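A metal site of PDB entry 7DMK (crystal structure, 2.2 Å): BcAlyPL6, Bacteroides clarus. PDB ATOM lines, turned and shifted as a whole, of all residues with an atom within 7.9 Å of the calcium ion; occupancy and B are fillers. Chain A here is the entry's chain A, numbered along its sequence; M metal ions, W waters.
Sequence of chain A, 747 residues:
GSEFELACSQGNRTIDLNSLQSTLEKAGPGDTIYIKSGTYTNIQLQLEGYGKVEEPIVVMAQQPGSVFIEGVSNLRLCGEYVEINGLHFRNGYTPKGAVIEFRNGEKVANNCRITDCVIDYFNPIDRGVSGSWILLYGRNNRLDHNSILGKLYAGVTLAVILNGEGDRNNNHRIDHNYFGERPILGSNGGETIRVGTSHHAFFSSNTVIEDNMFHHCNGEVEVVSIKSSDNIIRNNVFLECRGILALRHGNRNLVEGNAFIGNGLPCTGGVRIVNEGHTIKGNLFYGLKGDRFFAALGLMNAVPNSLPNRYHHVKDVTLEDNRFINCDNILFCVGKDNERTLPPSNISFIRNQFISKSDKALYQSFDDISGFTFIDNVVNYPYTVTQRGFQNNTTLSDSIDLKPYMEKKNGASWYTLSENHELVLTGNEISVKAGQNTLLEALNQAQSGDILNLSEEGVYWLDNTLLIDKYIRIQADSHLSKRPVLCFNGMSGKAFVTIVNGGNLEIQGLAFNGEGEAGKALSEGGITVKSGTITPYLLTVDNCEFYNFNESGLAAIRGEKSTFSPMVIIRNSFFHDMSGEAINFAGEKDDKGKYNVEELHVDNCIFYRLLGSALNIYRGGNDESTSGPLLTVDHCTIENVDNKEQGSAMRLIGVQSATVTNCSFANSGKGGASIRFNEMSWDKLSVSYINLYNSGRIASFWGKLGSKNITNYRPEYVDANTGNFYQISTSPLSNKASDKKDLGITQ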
ATOM      1  N   SER A 187      17.473  18.195 -11.435  1.00  0.00           N
ATOM      2  CA  SER A 187      18.923  18.095 -11.433  1.00  0.00           C
ATOM      3  C   SER A 187      19.332  17.338 -10.174  1.00  0.00           C
ATOM      4  O   SER A 187      18.496  17.031  -9.321  1.00  0.00           O
ATOM      5  CB  SER A 187      19.596  19.465 -11.469  1.00  0.00           C
ATOM      6  OG  SER A 187      19.497  20.117 -10.216  1.00  0.00           O
ATOM      7  N   ASN A 188      20.630  17.052 -10.075  1.00  0.00           N
ATOM      8  CA  ASN A 188      21.164  16.538  -8.822  1.00  0.00           C
ATOM      9  C   ASN A 188      21.201  17.658  -7.791  1.00  0.00           C
ATOM     10  O   ASN A 188      21.302  18.834  -8.122  1.00  0.00           O
ATOM     11  CB  ASN A 188      22.572  15.957  -9.026  1.00  0.00           C
ATOM     12  CG  ASN A 188      22.977  15.012  -7.910  1.00  0.00           C
ATOM     13  OD1 ASN A 188      22.224  14.776  -6.961  1.00  0.00           O
ATOM     14  ND2 ASN A 188      24.181  14.458  -8.007  1.00  0.00           N
ATOM     15  N   GLY A 189      21.105  17.272  -6.527  1.00  0.00           N
ATOM     16  CA  GLY A 189      21.107  18.217  -5.446  1.00  0.00           C
ATOM     17  C   GLY A 189      19.754  18.513  -4.837  1.00  0.00           C
ATOM     18  O   GLY A 189      19.552  19.625  -4.328  1.00  0.00           O
ATOM     19  N   GLY A 190      18.820  17.572  -4.888  1.00  0.00           N
ATOM     20  CA  GLY A 190      17.500  17.766  -4.311  1.00  0.00           C
ATOM     21  C   GLY A 190      17.171  16.789  -3.211  1.00  0.00           C
ATOM     22  O   GLY A 190      16.002  16.512  -2.945  1.00  0.00           O
ATOM     23  N   GLU A 191      18.209  16.247  -2.558  1.00  0.00           N
ATOM     24  CA  GLU A 191      18.009  15.323  -1.459  1.00  0.00           C
ATOM     25  C   GLU A 191      17.267  15.993  -0.304  1.00  0.00           C
ATOM     26  O   GLU A 191      17.352  17.208  -0.105  1.00  0.00           O
ATOM     27  CB  GLU A 191      19.349  14.780  -0.961  1.00  0.00           C
ATOM     28  CG  GLU A 191      20.246  14.187  -2.040  1.00  0.00           C
ATOM     29  CD  GLU A 191      21.233  15.202  -2.588  1.00  0.00           C
ATOM     30  OE1 GLU A 191      20.962  16.414  -2.480  1.00  0.00           O
ATOM     31  OE2 GLU A 191      22.276  14.786  -3.129  1.00  0.00           O
ATOM     32  N   ARG A 194      21.039  14.227   3.730  1.00  0.00           N
ATOM     33  CA  ARG A 194      22.340  13.689   3.363  1.00  0.00           C
ATOM     34  C   ARG A 194      23.190  13.567   4.610  1.00  0.00           C
ATOM     35  O   ARG A 194      23.314  14.529   5.384  1.00  0.00           O
ATOM     36  CB  ARG A 194      23.040  14.592   2.331  1.00  0.00           C
ATOM     37  CG  ARG A 194      24.311  13.971   1.745  1.00  0.00           C
ATOM     38  CD  ARG A 194      25.181  15.004   1.043  1.00  0.00           C
ATOM     39  NE  ARG A 194      25.869  15.874   1.981  1.00  0.00           N
ATOM     40  CZ  ARG A 194      25.933  17.196   1.879  1.00  0.00           C
ATOM     41  NH1 ARG A 194      25.348  17.818   0.868  1.00  0.00           N
ATOM     42  NH2 ARG A 194      26.593  17.910   2.793  1.00  0.00           N
ATOM     43  N   GLU A 220      14.879  14.433  -6.129  1.00  0.00           N
ATOM     44  CA  GLU A 220      15.769  13.704  -7.027  1.00  0.00           C
ATOM     45  C   GLU A 220      15.664  12.219  -6.697  1.00  0.00           C
ATOM     46  O   GLU A 220      14.752  11.804  -5.973  1.00  0.00           O
ATOM     47  CB  GLU A 220      17.203  14.233  -6.915  1.00  0.00           C
ATOM     48  CG  GLU A 220      17.718  14.247  -5.483  1.00  0.00           C
ATOM     49  CD  GLU A 220      19.201  13.970  -5.401  1.00  0.00           C
ATOM     50  OE1 GLU A 220      19.593  12.788  -5.397  1.00  0.00           O
ATOM     51  OE2 GLU A 220      19.970  14.951  -5.350  1.00  0.00           O
ATOM     52  N   VAL A 221      16.614  11.430  -7.203  1.00  0.00           N
ATOM     53  CA  VAL A 221      16.582   9.989  -6.967  1.00  0.00           C
ATOM     54  C   VAL A 221      16.784   9.681  -5.480  1.00  0.00           C
ATOM     55  O   VAL A 221      16.148   8.773  -4.941  1.00  0.00           O
ATOM     56  CB  VAL A 221      17.624   9.266  -7.839  1.00  0.00           C
ATOM     57  CG1 VAL A 221      19.052   9.639  -7.440  1.00  0.00           C
ATOM     58  CG2 VAL A 221      17.415   7.762  -7.784  1.00  0.00           C
ATOM     59  N   GLU A 222      17.626  10.447  -4.797  1.00  0.00           N
ATOM     60  CA  GLU A 222      17.940  10.195  -3.394  1.00  0.00           C
ATOM     61  C   GLU A 222      17.021  11.032  -2.514  1.00  0.00           C
ATOM     62  O   GLU A 222      17.172  12.260  -2.437  1.00  0.00           O
ATOM     63  CB  GLU A 222      19.399  10.524  -3.091  1.00  0.00           C
ATOM     64  CG  GLU A 222      20.420   9.662  -3.807  1.00  0.00           C
ATOM     65  CD  GLU A 222      21.848  10.063  -3.469  1.00  0.00           C
ATOM     66  OE1 GLU A 222      22.138  11.278  -3.438  1.00  0.00           O
ATOM     67  OE2 GLU A 222      22.687   9.166  -3.234  1.00  0.00           O
ATOM     68  N   VAL A 223      16.076  10.367  -1.839  1.00  0.00           N
ATOM     69  CA  VAL A 223      15.359  11.030  -0.746  1.00  0.00           C
ATOM     70  C   VAL A 223      16.288  11.205   0.436  1.00  0.00           C
ATOM     71  O   VAL A 223      16.436  12.312   0.983  1.00  0.00           O
ATOM     72  CB  VAL A 223      14.102  10.227  -0.374  1.00  0.00           C
ATOM     73  CG1 VAL A 223      13.400  10.873   0.829  1.00  0.00           C
ATOM     74  CG2 VAL A 223      13.167  10.124  -1.560  1.00  0.00           C
ATOM     75  N   VAL A 224      16.935  10.120   0.863  1.00  0.00           N
ATOM     76  CA  VAL A 224      17.966  10.142   1.894  1.00  0.00           C
ATOM     77  C   VAL A 224      19.237   9.597   1.278  1.00  0.00           C
ATOM     78  O   VAL A 224      19.235   8.499   0.690  1.00  0.00           O
ATOM     79  CB  VAL A 224      17.549   9.314   3.125  1.00  0.00           C
ATOM     80  CG1 VAL A 224      18.694   9.260   4.131  1.00  0.00           C
ATOM     81  CG2 VAL A 224      16.287   9.892   3.756  1.00  0.00           C
ATOM     82  N   SER A 225      20.325  10.350   1.396  1.00  0.00           N
ATOM     83  CA  SER A 225      21.622   9.966   0.841  1.00  0.00           C
ATOM     84  C   SER A 225      22.569   9.705   1.998  1.00  0.00           C
ATOM     85  O   SER A 225      23.040  10.636   2.651  1.00  0.00           O
ATOM     86  CB  SER A 225      22.152  11.057  -0.086  1.00  0.00           C
ATOM     87  OG  SER A 225      23.424  10.726  -0.608  1.00  0.00           O
ATOM     88  N   LYS A 227      26.051   8.831   3.114  1.00  0.00           N
ATOM     89  CA  LYS A 227      27.430   8.872   2.619  1.00  0.00           C
ATOM     90  C   LYS A 227      28.409   8.853   3.779  1.00  0.00           C
ATOM     91  O   LYS A 227      29.382   9.608   3.814  1.00  0.00           O
ATOM     92  CB  LYS A 227      27.646  10.087   1.726  1.00  0.00           C
ATOM     93  CG  LYS A 227      26.868  10.027   0.419  1.00  0.00           C
ATOM     94  CD  LYS A 227      27.012  11.306  -0.391  1.00  0.00           C
ATOM     95  CE  LYS A 227      26.520  11.088  -1.816  1.00  0.00           C
ATOM     96  NZ  LYS A 227      26.568  12.345  -2.614  1.00  0.00           N
ATOM     97  N   ALA A 246      19.246   5.790  -0.266  1.00  0.00           N
ATOM     98  CA  ALA A 246      20.477   5.441  -0.961  1.00  0.00           C
ATOM     99  C   ALA A 246      21.593   5.208   0.046  1.00  0.00           C
ATOM    100  O   ALA A 246      21.996   6.130   0.764  1.00  0.00           O
ATOM    101  CB  ALA A 246      20.878   6.537  -1.952  1.00  0.00           C
ATOM    102  N   ARG A 248      24.799   5.183  -0.382  1.00  0.00           N
ATOM    103  CA  ARG A 248      25.623   5.606  -1.497  1.00  0.00           C
ATOM    104  C   ARG A 248      27.106   5.477  -1.185  1.00  0.00           C
ATOM    105  O   ARG A 248      27.879   4.921  -1.984  1.00  0.00           O
ATOM    106  CB  ARG A 248      25.273   7.050  -1.880  1.00  0.00           C
ATOM    107  CG  ARG A 248      26.083   7.620  -3.025  1.00  0.00           C
ATOM    108  CD  ARG A 248      25.862   6.855  -4.322  1.00  0.00           C
ATOM    109  NE  ARG A 248      26.737   7.364  -5.383  1.00  0.00           N
ATOM    110  CZ  ARG A 248      27.996   6.975  -5.565  1.00  0.00           C
ATOM    111  NH1 ARG A 248      28.540   6.053  -4.767  1.00  0.00           N
ATOM    112  NH2 ARG A 248      28.710   7.498  -6.555  1.00  0.00           N
ATOM    113  N   ARG A 272      18.604   1.566  -2.701  1.00  0.00           N
ATOM    114  CA  ARG A 272      19.707   1.304  -3.644  1.00  0.00           C
ATOM    115  C   ARG A 272      20.955   1.097  -2.787  1.00  0.00           C
ATOM    116  O   ARG A 272      21.199   1.890  -1.927  1.00  0.00           O
ATOM    117  CB  ARG A 272      19.859   2.388  -4.719  1.00  0.00           C
ATOM    118  CG  ARG A 272      20.997   2.129  -5.683  1.00  0.00           C
ATOM    119  CD  ARG A 272      20.756   2.738  -7.026  1.00  0.00           C
ATOM    120  NE  ARG A 272      20.371   4.118  -6.973  1.00  0.00           N
ATOM    121  CZ  ARG A 272      21.228   5.107  -6.916  1.00  0.00           C
ATOM    122  NH1 ARG A 272      22.522   4.862  -6.935  1.00  0.00           N
ATOM    123  NH2 ARG A 272      20.815   6.338  -6.843  1.00  0.00           N
ATOM    124  N   ASP A 623      24.702  12.541 -15.801  1.00  0.00           N
ATOM    125  CA  ASP A 623      24.191  12.452 -14.438  1.00  0.00           C
ATOM    126  C   ASP A 623      23.128  11.369 -14.328  1.00  0.00           C
ATOM    127  O   ASP A 623      22.287  11.207 -15.225  1.00  0.00           O
ATOM    128  CB  ASP A 623      23.608  13.781 -13.983  1.00  0.00           C
ATOM    129  CG  ASP A 623      22.790  13.652 -12.714  1.00  0.00           C
ATOM    130  OD1 ASP A 623      23.395  13.590 -11.620  1.00  0.00           O
ATOM    131  OD2 ASP A 623      21.548  13.596 -12.800  1.00  0.00           O
ATOM    132  N   GLU A 624      23.163  10.618 -13.222  1.00  0.00           N
ATOM    133  CA  GLU A 624      22.244   9.517 -12.974  1.00  0.00           C
ATOM    134  C   GLU A 624      21.321   9.805 -11.790  1.00  0.00           C
ATOM    135  O   GLU A 624      20.865   8.870 -11.121  1.00  0.00           O
ATOM    136  CB  GLU A 624      23.024   8.220 -12.744  1.00  0.00           C
ATOM    137  CG  GLU A 624      23.917   7.814 -13.910  1.00  0.00           C
ATOM    138  CD  GLU A 624      24.709   6.537 -13.631  1.00  0.00           C
ATOM    139  OE1 GLU A 624      25.578   6.549 -12.724  1.00  0.00           O
ATOM    140  OE2 GLU A 624      24.448   5.521 -14.319  1.00  0.00           O
ATOM    141  N   SER A 625      21.026  11.079 -11.523  1.00  0.00           N
ATOM    142  CA  SER A 625      20.327  11.481 -10.309  1.00  0.00           C
ATOM    143  C   SER A 625      18.868  11.853 -10.532  1.00  0.00           C
ATOM    144  O   SER A 625      18.172  12.152  -9.554  1.00  0.00           O
ATOM    145  CB  SER A 625      21.049  12.664  -9.656  1.00  0.00           C
ATOM    146  OG  SER A 625      22.356  12.309  -9.251  1.00  0.00           O
ATOM    147  N   THR A 626      18.377  11.840 -11.768  1.00  0.00           N
ATOM    148  CA  THR A 626      17.032  12.319 -12.058  1.00  0.00           C
ATOM    149  C   THR A 626      16.224  11.252 -12.777  1.00  0.00           C
ATOM    150  O   THR A 626      16.739  10.191 -13.173  1.00  0.00           O
ATOM    151  CB  THR A 626      17.057  13.594 -12.902  1.00  0.00           C
ATOM    152  OG1 THR A 626      17.642  13.318 -14.179  1.00  0.00           O
ATOM    153  CG2 THR A 626      17.842  14.698 -12.197  1.00  0.00           C
HETATM  154 CA    CA M   1      22.040  13.105  -5.176  1.00  0.00          CA
HETATM  155  O   HOH W   1      22.445  11.287  -6.889  1.00  0.00           O
HETATM  156  O   HOH W   2      24.492  13.237  -5.220  1.00  0.00           O
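The side-chain carboxylate (OE2) of Glu 222 is in hydrogen-bond range of the side-chain hydroxyl (OG) of Ser 225, 3.1 Å away. ND2 of Asn 188 sits close to OG of Ser 625, 3.1 Å away. The backbone NH of Gly 190 lies close to the side-chain carboxylate of Glu 220 (2.9 Å). The side-chain carboxylate (OE2) of Glu 220 sits close to the backbone NH (N) of Gly 189 (2.8 Å).
The calcium ion is bound by the side-chain amide oxygen (OD1) of Asn 188 (2.5 Å), water W2 (2.5 Å), the side-chain carboxylate (OE1) of Glu 220 (2.5 Å), the side-chain carboxylate (OE1) of Glu 222 (2.5 Å), water W1 (2.5 Å), the side-chain carboxylate (OE2) of Glu 191 (2.7 Å) and the side-chain carboxylate (OE2) of Glu 220 (2.8 Å).
Water W2 lies within hydrogen-bond range of the side-chain amide nitrogen (ND2) of Asn 188 and the side-chain amino group (NZ) of Lys 227.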
